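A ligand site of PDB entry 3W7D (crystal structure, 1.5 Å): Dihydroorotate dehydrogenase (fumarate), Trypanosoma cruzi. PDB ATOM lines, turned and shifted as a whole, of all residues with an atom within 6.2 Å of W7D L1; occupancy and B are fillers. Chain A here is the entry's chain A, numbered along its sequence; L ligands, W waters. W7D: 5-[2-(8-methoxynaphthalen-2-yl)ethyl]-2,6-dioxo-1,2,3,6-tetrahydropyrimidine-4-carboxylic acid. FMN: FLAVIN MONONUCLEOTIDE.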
ATOM      1  N   ALA A  20       2.276  -4.403  -1.219  1.00  0.00           N
ATOM      2  CA  ALA A  20       3.107  -5.504  -0.910  1.00  0.00           C
ATOM      3  C   ALA A  20       3.251  -5.609   0.600  1.00  0.00           C
ATOM      4  O   ALA A  20       3.387  -4.650   1.361  1.00  0.00           O
ATOM      5  CB  ALA A  20       4.481  -5.344  -1.544  1.00  0.00           C
ATOM      6  N   LYS A  44       4.224 -10.773  -1.218  1.00  0.00           N
ATOM      7  CA  LYS A  44       5.117 -10.329  -0.215  1.00  0.00           C
ATOM      8  C   LYS A  44       6.534 -10.215  -0.697  1.00  0.00           C
ATOM      9  O   LYS A  44       7.022 -11.128  -1.334  1.00  0.00           O
ATOM     10  CB  LYS A  44       5.077 -11.280   0.989  1.00  0.00           C
ATOM     11  CG  LYS A  44       6.122 -11.017   2.049  1.00  0.00           C
ATOM     12  CD  LYS A  44       5.994  -9.711   2.847  1.00  0.00           C
ATOM     13  CE  LYS A  44       7.262  -9.337   3.641  1.00  0.00           C
ATOM     14  NZ  LYS A  44       7.020  -8.080   4.473  1.00  0.00           N
ATOM     15  N   SER A  45       7.170  -9.120  -0.373  1.00  0.00           N
ATOM     16  CA  SER A  45       8.578  -8.974  -0.820  1.00  0.00           C
ATOM     17  C   SER A  45       9.378 -10.167  -0.304  1.00  0.00           C
ATOM     18  O   SER A  45       9.364 -10.486   0.882  1.00  0.00           O
ATOM     19  CB  SER A  45       9.226  -7.751  -0.235  1.00  0.00           C
ATOM     20  OG  SER A  45       8.788  -6.565  -0.869  1.00  0.00           O
ATOM     21  N   ARG A  51      12.530 -16.471   5.520  1.00  0.00           N
ATOM     22  CA  ARG A  51      12.962 -15.706   6.692  1.00  0.00           C
ATOM     23  C   ARG A  51      11.934 -15.678   7.824  1.00  0.00           C
ATOM     24  O   ARG A  51      10.758 -15.404   7.604  1.00  0.00           O
ATOM     25  CB  ARG A  51      13.323 -14.273   6.280  1.00  0.00           C
ATOM     26  CG  ARG A  51      14.566 -14.162   5.416  1.00  0.00           C
ATOM     27  CD  ARG A  51      14.922 -12.711   5.145  1.00  0.00           C
ATOM     28  NE  ARG A  51      14.607 -11.852   6.277  1.00  0.00           N
ATOM     29  CZ  ARG A  51      15.500 -11.452   7.185  1.00  0.00           C
ATOM     30  NH1 ARG A  51      16.768 -11.839   7.081  1.00  0.00           N
ATOM     31  NH2 ARG A  51      15.131 -10.670   8.186  1.00  0.00           N
ATOM     32  N   ASN A  54      11.495 -10.404  12.210  1.00  0.00           N
ATOM     33  CA  ASN A  54      11.643  -9.793  13.527  1.00  0.00           C
ATOM     34  C   ASN A  54      10.631 -10.290  14.563  1.00  0.00           C
ATOM     35  O   ASN A  54       9.496 -10.623  14.217  1.00  0.00           O
ATOM     36  CB  ASN A  54      11.568  -8.264  13.425  1.00  0.00           C
ATOM     37  CG  ASN A  54      12.691  -7.675  12.597  1.00  0.00           C
ATOM     38  OD1 ASN A  54      13.743  -8.302  12.425  1.00  0.00           O
ATOM     39  ND2 ASN A  54      12.485  -6.474  12.084  1.00  0.00           N
ATOM     40  N   ASN A  68       5.045  -0.749  11.659  1.00  0.00           N
ATOM     41  CA  ASN A  68       5.514  -2.092  11.509  1.00  0.00           C
ATOM     42  C   ASN A  68       7.034  -2.119  11.400  1.00  0.00           C
ATOM     43  O   ASN A  68       7.685  -1.267  10.825  1.00  0.00           O
ATOM     44  CB  ASN A  68       4.907  -2.847  10.290  1.00  0.00           C
ATOM     45  CG  ASN A  68       5.638  -2.593   9.029  1.00  0.00           C
ATOM     46  OD1 ASN A  68       6.649  -3.281   8.703  1.00  0.00           O
ATOM     47  ND2 ASN A  68       5.176  -1.692   8.237  1.00  0.00           N
ATOM     48  N   SER A  69       7.606  -3.165  11.977  1.00  0.00           N
ATOM     49  CA  SER A  69       8.942  -3.626  11.632  1.00  0.00           C
ATOM     50  C   SER A  69       8.923  -5.139  11.431  1.00  0.00           C
ATOM     51  O   SER A  69       9.414  -5.861  12.231  1.00  0.00           O
ATOM     52  CB  SER A  69       9.931  -3.232  12.725  1.00  0.00           C
ATOM     53  OG  SER A  69      11.220  -3.539  12.321  1.00  0.00           O
ATOM     54  N   MET A  70       8.292  -5.567  10.358  1.00  0.00           N
ATOM     55  CA  MET A  70       8.134  -6.993  10.100  1.00  0.00           C
ATOM     56  C   MET A  70       9.441  -7.754   9.921  1.00  0.00           C
ATOM     57  O   MET A  70       9.581  -8.813  10.409  1.00  0.00           O
ATOM     58  CB  MET A  70       7.272  -7.234   8.869  1.00  0.00           C
ATOM     59  CG  MET A  70       5.944  -6.555   8.828  1.00  0.00           C
ATOM     60  SD  MET A  70       4.907  -6.957  10.263  1.00  0.00           S
ATOM     61  CE  MET A  70       4.405  -8.634   9.872  1.00  0.00           C
ATOM     62  N   GLY A  71      10.380  -7.143   9.236  1.00  0.00           N
ATOM     63  CA  GLY A  71      11.639  -7.797   9.017  1.00  0.00           C
ATOM     64  C   GLY A  71      11.699  -8.809   7.897  1.00  0.00           C
ATOM     65  O   GLY A  71      12.387  -9.741   7.993  1.00  0.00           O
ATOM     66  N   LEU A  72      10.859  -8.579   6.714  1.00  0.00           N
ATOM     67  CA  LEU A  72      10.796  -9.552   5.641  1.00  0.00           C
ATOM     68  C   LEU A  72      10.575 -11.016   6.086  1.00  0.00           C
ATOM     69  O   LEU A  72      11.171 -11.874   5.584  1.00  0.00           O
ATOM     70  CB  LEU A  72      12.074  -9.475   4.813  1.00  0.00           C
ATOM     71  CG  LEU A  72      12.308  -8.165   4.053  1.00  0.00           C
ATOM     72  CD1 LEU A  72      13.679  -8.164   3.394  1.00  0.00           C
ATOM     73  CD2 LEU A  72      11.215  -7.941   3.024  1.00  0.00           C
ATOM     74  N   PRO A  73       9.567 -11.199   6.857  1.00  0.00           N
ATOM     75  CA  PRO A  73       9.154 -12.576   6.969  1.00  0.00           C
ATOM     76  C   PRO A  73       8.561 -13.037   5.637  1.00  0.00           C
ATOM     77  O   PRO A  73       7.734 -12.398   5.142  1.00  0.00           O
ATOM     78  CB  PRO A  73       8.080 -12.536   8.033  1.00  0.00           C
ATOM     79  CG  PRO A  73       7.549 -11.147   8.037  1.00  0.00           C
ATOM     80  CD  PRO A  73       8.594 -10.264   7.408  1.00  0.00           C
ATOM     81  N   SER A 100      12.871  -8.339  -2.640  1.00  0.00           N
ATOM     82  CA  SER A 100      13.639  -7.458  -1.740  1.00  0.00           C
ATOM     83  C   SER A 100      14.829  -8.157  -1.183  1.00  0.00           C
ATOM     84  O   SER A 100      15.026  -8.288   0.049  1.00  0.00           O
ATOM     85  CB  SER A 100      12.709  -6.967  -0.649  1.00  0.00           C
ATOM     86  OG  SER A 100      13.342  -6.127   0.255  1.00  0.00           O
ATOM     87  N   LEU A 102      18.666  -8.677   0.040  1.00  0.00           N
ATOM     88  CA  LEU A 102      19.431  -7.988   1.064  1.00  0.00           C
ATOM     89  C   LEU A 102      20.792  -7.487   0.578  1.00  0.00           C
ATOM     90  O   LEU A 102      21.516  -6.794   1.331  1.00  0.00           O
ATOM     91  CB  LEU A 102      19.493  -8.848   2.356  1.00  0.00           C
ATOM     92  CG  LEU A 102      18.040  -8.982   2.949  1.00  0.00           C
ATOM     93  CD1 LEU A 102      18.183 -10.078   3.993  1.00  0.00           C
ATOM     94  CD2 LEU A 102      17.464  -7.743   3.515  1.00  0.00           C
ATOM     95  N   ASN A 128      11.690  -3.886  -4.712  1.00  0.00           N
ATOM     96  CA  ASN A 128      11.596  -3.048  -3.554  1.00  0.00           C
ATOM     97  C   ASN A 128      12.929  -2.353  -3.274  1.00  0.00           C
ATOM     98  O   ASN A 128      13.862  -2.998  -2.812  1.00  0.00           O
ATOM     99  CB  ASN A 128      11.160  -3.912  -2.356  1.00  0.00           C
ATOM    100  CG  ASN A 128      10.965  -3.085  -1.126  1.00  0.00           C
ATOM    101  OD1 ASN A 128      10.962  -1.900  -1.112  1.00  0.00           O
ATOM    102  ND2 ASN A 128      10.524  -3.823  -0.113  1.00  0.00           N
ATOM    103  N   SER A 130      13.380  -0.137  -0.928  1.00  0.00           N
ATOM    104  CA  SER A 130      13.688  -0.220   0.507  1.00  0.00           C
ATOM    105  C   SER A 130      14.436  -1.487   1.081  1.00  0.00           C
ATOM    106  O   SER A 130      14.563  -1.636   2.230  1.00  0.00           O
ATOM    107  CB  SER A 130      12.480   0.111   1.303  1.00  0.00           C
ATOM    108  OG  SER A 130      11.964   1.370   0.847  1.00  0.00           O
ATOM    109  N   CYS A 131      14.942  -2.391   0.221  1.00  0.00           N
ATOM    110  CA  CYS A 131      15.639  -3.543   0.686  1.00  0.00           C
ATOM    111  C   CYS A 131      16.782  -2.919   1.544  1.00  0.00           C
ATOM    112  O   CYS A 131      17.240  -1.787   1.325  1.00  0.00           O
ATOM    113  CB  CYS A 131      16.145  -4.348  -0.498  1.00  0.00           C
ATOM    114  SG  CYS A 131      16.934  -3.413  -1.864  1.00  0.00           S
ATOM    115  N   PRO A 132      17.099  -3.604   2.611  1.00  0.00           N
ATOM    116  CA  PRO A 132      18.039  -2.993   3.553  1.00  0.00           C
ATOM    117  C   PRO A 132      19.313  -3.009   2.798  1.00  0.00           C
ATOM    118  O   PRO A 132      19.413  -3.815   1.998  1.00  0.00           O
ATOM    119  CB  PRO A 132      18.045  -3.977   4.733  1.00  0.00           C
ATOM    120  CG  PRO A 132      17.000  -5.000   4.458  1.00  0.00           C
ATOM    121  CD  PRO A 132      16.227  -4.600   3.240  1.00  0.00           C
ATOM    122  N   LYS A 165       9.453  -0.109  -6.168  1.00  0.00           N
ATOM    123  CA  LYS A 165       8.748   0.445  -4.997  1.00  0.00           C
ATOM    124  C   LYS A 165       9.671   1.390  -4.288  1.00  0.00           C
ATOM    125  O   LYS A 165      10.792   1.018  -3.898  1.00  0.00           O
ATOM    126  CB  LYS A 165       8.359  -0.687  -4.089  1.00  0.00           C
ATOM    127  CG  LYS A 165       7.655  -0.286  -2.777  1.00  0.00           C
ATOM    128  CD  LYS A 165       6.204   0.109  -2.988  1.00  0.00           C
ATOM    129  CE  LYS A 165       5.420   0.246  -1.721  1.00  0.00           C
ATOM    130  NZ  LYS A 165       5.142  -1.065  -1.150  1.00  0.00           N
ATOM    131  N   ASN A 195       6.328   3.467  -0.220  1.00  0.00           N
ATOM    132  CA  ASN A 195       6.549   2.642   0.982  1.00  0.00           C
ATOM    133  C   ASN A 195       6.467   3.429   2.292  1.00  0.00           C
ATOM    134  O   ASN A 195       6.480   4.656   2.295  1.00  0.00           O
ATOM    135  CB  ASN A 195       7.969   1.986   0.926  1.00  0.00           C
ATOM    136  CG  ASN A 195       7.995   0.555   1.446  1.00  0.00           C
ATOM    137  OD1 ASN A 195       7.503   0.276   2.536  1.00  0.00           O
ATOM    138  ND2 ASN A 195       8.654  -0.341   0.723  1.00  0.00           N
ATOM    139  N   SER A 196       6.378   2.708   3.407  1.00  0.00           N
ATOM    140  CA  SER A 196       6.076   3.295   4.703  1.00  0.00           C
ATOM    141  C   SER A 196       6.999   4.449   5.067  1.00  0.00           C
ATOM    142  O   SER A 196       8.202   4.415   4.806  1.00  0.00           O
ATOM    143  CB  SER A 196       6.118   2.220   5.795  1.00  0.00           C
ATOM    144  OG  SER A 196       7.169   1.303   5.561  1.00  0.00           O
ATOM    145  N   LYS A 215      13.706  -2.883  17.161  1.00  0.00           N
ATOM    146  CA  LYS A 215      14.278  -1.570  16.921  1.00  0.00           C
ATOM    147  C   LYS A 215      13.796  -0.580  17.953  1.00  0.00           C
ATOM    148  O   LYS A 215      13.587   0.619  17.645  1.00  0.00           O
ATOM    149  CB  LYS A 215      13.966  -1.091  15.483  1.00  0.00           C
ATOM    150  CG  LYS A 215      14.542  -1.934  14.371  1.00  0.00           C
ATOM    151  CD  LYS A 215      14.067  -1.386  13.017  1.00  0.00           C
ATOM    152  CE  LYS A 215      14.169   0.124  12.784  1.00  0.00           C
ATOM    153  NZ  LYS A 215      14.111   0.510  11.335  1.00  0.00           N
ATOM    154  N   GLY A 220       8.085   1.513  10.381  1.00  0.00           N
ATOM    155  CA  GLY A 220       7.507   2.272   9.302  1.00  0.00           C
ATOM    156  C   GLY A 220       6.017   2.512   9.484  1.00  0.00           C
ATOM    157  O   GLY A 220       5.292   1.693   9.912  1.00  0.00           O
HETATM  158  O   W7D L   1       9.135  -6.497   5.938  1.00  0.00           O
HETATM  159  C   W7D L   1       9.173  -5.326   6.374  1.00  0.00           C
HETATM  160  OXT W7D L   1       9.406  -4.936   7.516  1.00  0.00           O
HETATM  161  CA  W7D L   1       8.744  -4.253   5.388  1.00  0.00           C
HETATM  162  N   W7D L   1       7.828  -3.315   5.953  1.00  0.00           N
HETATM  163  CAR W7D L   1       7.443  -2.221   5.249  1.00  0.00           C
HETATM  164  OAC W7D L   1       6.631  -1.402   5.704  1.00  0.00           O
HETATM  165  ND2 W7D L   1       7.998  -2.024   4.024  1.00  0.00           N
HETATM  166  CG  W7D L   1       8.950  -2.852   3.391  1.00  0.00           C
HETATM  167  OD1 W7D L   1       9.373  -2.658   2.245  1.00  0.00           O
HETATM  168  CB  W7D L   1       9.302  -4.020   4.114  1.00  0.00           C
HETATM  169  CAM W7D L   1      10.410  -4.901   3.654  1.00  0.00           C
HETATM  170  CAL W7D L   1      11.805  -4.201   3.651  1.00  0.00           C
HETATM  171  CAT W7D L   1      12.245  -4.058   4.972  1.00  0.00           C
HETATM  172  CAK W7D L   1      13.141  -4.956   5.641  1.00  0.00           C
HETATM  173  CAW W7D L   1      13.516  -4.759   7.052  1.00  0.00           C
HETATM  174  CAH W7D L   1      11.796  -2.931   5.711  1.00  0.00           C
HETATM  175  CAJ W7D L   1      12.123  -2.803   7.099  1.00  0.00           C
HETATM  176  CAV W7D L   1      12.979  -3.673   7.747  1.00  0.00           C
HETATM  177  CAI W7D L   1      13.293  -3.438   9.140  1.00  0.00           C
HETATM  178  CAF W7D L   1      14.158  -4.364   9.684  1.00  0.00           C
HETATM  179  CAG W7D L   1      14.710  -5.455   9.031  1.00  0.00           C
HETATM  180  CAU W7D L   1      14.425  -5.654   7.636  1.00  0.00           C
HETATM  181  OAP W7D L   1      14.820  -6.657   6.875  1.00  0.00           O
HETATM  182  CAA W7D L   1      15.770  -7.580   7.513  1.00  0.00           C
HETATM  183  N1  FMN L   2       6.178  -2.825   1.282  1.00  0.00           N
HETATM  184  C2  FMN L   2       6.948  -3.587   0.434  1.00  0.00           C
HETATM  185  O2  FMN L   2       7.274  -3.066  -0.655  1.00  0.00           O
HETATM  186  N3  FMN L   2       7.248  -4.865   0.721  1.00  0.00           N
HETATM  187  C4  FMN L   2       6.823  -5.494   1.820  1.00  0.00           C
HETATM  188  O4  FMN L   2       7.083  -6.710   2.028  1.00  0.00           O
HETATM  189  C4A FMN L   2       6.054  -4.742   2.762  1.00  0.00           C
HETATM  190  N5  FMN L   2       5.582  -5.339   3.852  1.00  0.00           N
HETATM  191  C5A FMN L   2       4.689  -4.661   4.640  1.00  0.00           C
HETATM  192  C6  FMN L   2       4.079  -5.281   5.728  1.00  0.00           C
HETATM  193  C7  FMN L   2       3.144  -4.621   6.515  1.00  0.00           C
HETATM  194  C7M FMN L   2       2.481  -5.293   7.687  1.00  0.00           C
HETATM  195  C8  FMN L   2       2.803  -3.291   6.209  1.00  0.00           C
HETATM  196  C8M FMN L   2       1.794  -2.520   7.008  1.00  0.00           C
HETATM  197  C9  FMN L   2       3.399  -2.665   5.145  1.00  0.00           C
HETATM  198  C9A FMN L   2       4.337  -3.301   4.336  1.00  0.00           C
HETATM  199  N10 FMN L   2       4.913  -2.633   3.217  1.00  0.00           N
HETATM  200  C10 FMN L   2       5.749  -3.370   2.439  1.00  0.00           C
HETATM  201  C1' FMN L   2       4.571  -1.250   2.912  1.00  0.00           C
HETATM  202  C2' FMN L   2       3.246  -1.172   2.178  1.00  0.00           C
HETATM  203  O2' FMN L   2       3.360  -1.898   0.935  1.00  0.00           O
HETATM  204  C3' FMN L   2       2.841   0.235   1.907  1.00  0.00           C
HETATM  205  O3' FMN L   2       3.871   0.776   1.017  1.00  0.00           O
HETATM  206  C4' FMN L   2       2.771   1.114   3.199  1.00  0.00           C
HETATM  207  O4' FMN L   2       2.103   0.312   4.222  1.00  0.00           O
HETATM  208  C5' FMN L   2       1.873   2.367   2.894  1.00  0.00           C
HETATM  209  O5' FMN L   2       0.581   2.077   2.436  1.00  0.00           O
HETATM  210  P   FMN L   2      -0.686   2.204   3.437  1.00  0.00           P
HETATM  211  O1P FMN L   2      -1.870   1.786   2.576  1.00  0.00           O
HETATM  212  O2P FMN L   2      -0.701   3.611   3.929  1.00  0.00           O
HETATM  213  O3P FMN L   2      -0.392   1.213   4.592  1.00  0.00           O
HETATM  214  O   HOH W   1       9.314  -2.110   8.380  1.00  0.00           O
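A nitrogen (N1) of FMN L2 lies close to a nitrogen (ND2) of W7D L1, at 3.4 Å.
The backbone NH of Gly 220 sits at hydrogen-bond distance from the backbone carbonyl oxygen of Asn 68 (2.8 Å). ND2 of Asn 195 sits at hydrogen-bond distance from OD1 of Asn 128. NH2 of Arg 51 is in hydrogen-bond range of O of Gly 71 (2.9 Å). ND2 of Asn 128 sits at hydrogen-bond distance from OG of Ser 45, 3.3 Å away. O of Ser 69 lies within hydrogen-bond range of ND2 of Asn 54 (3.1 Å). O of Met 70 lies within hydrogen-bond range of N of Asn 54 (3.1 Å). O of Asn 128 lies within hydrogen-bond range of SG of Cys 131 (3.2 Å). The side-chain amide oxygen of Asn 128 is in hydrogen-bond range of the backbone NH of Ser 130, 3.0 Å away.
ND2 of Asn 128 lies within hydrogen-bond range of OD1 of W7D L1, at 2.9 Å. The backbone NH (N) of Ser 45 lies close to an oxygen (O4) of FMN L2, at 3.4 Å. The side-chain amide nitrogen (ND2) of Asn 128 sits at hydrogen-bond distance from an oxygen (O2) of FMN L2 (3.4 Å). ND2 of Asn 195 sits at hydrogen-bond distance from O2 of FMN L2 (3.4 Å). N3 of FMN L2 lies within hydrogen-bond range of OG of Ser 45, at 2.8 Å. The side-chain amino group (NZ) of Lys 44 is in salt-bridge range of an oxygen (O) of W7D L1, 3.0 Å away. An oxygen (O2') of FMN L2 is in hydrogen-bond range of the backbone NH (N) of Ala 20, at 3.5 Å. An oxygen (OXT) of W7D L1 is in hydrogen-bond range of the backbone NH of Met 70 (3.1 Å). O2' of FMN L2 lies within hydrogen-bond range of NZ of Lys 165, at 2.9 Å. The side-chain amide oxygen (OD1) of Asn 195 is in hydrogen-bond range of a nitrogen (ND2) of W7D L1, at 2.8 Å. The backbone NH of Gly 71 lies within hydrogen-bond range of an oxygen (OXT) of W7D L1, 3.0 Å away. N of Leu 72 lies within hydrogen-bond range of O of W7D L1 (2.8 Å). O of Ala 20 lies within hydrogen-bond range of O2' of FMN L2 (2.8 Å). An oxygen (O4) of FMN L2 lies within hydrogen-bond range of the side-chain amino group (NZ) of Lys 44 (2.8 Å). An oxygen (OAC) of W7D L1 sits at hydrogen-bond distance from the side-chain amide nitrogen (ND2) of Asn 68 (2.9 Å). OAC of W7D L1 sits at hydrogen-bond distance from OG of Ser 196 (2.8 Å).
Water W1 bridges the side-chain amide oxygen of Asn 68 and an oxygen (OXT) of W7D L1.
NH2 of Arg 51 touches CAA of W7D L1 (3.2 Å). ND2 of Asn 54 touches CAF of W7D L1, 3.6 Å away. Ser 69 touches W7D L1. Pro 132 touches W7D L1. Hydrophobic or aromatic side chains that line W7D L1: Met 70, Leu 72 and Pro 132. 12 residues have an atom within 4 Å of W7D L1: Lys 44, Arg 51, Asn 54, Asn 68, Ser 69, Met 70, Gly 71, Leu 72, Asn 128, Pro 132, Asn 195 and Ser 196. The nearest printed residue that does not touch W7D L1 is Ser 130 (4.03 Å).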
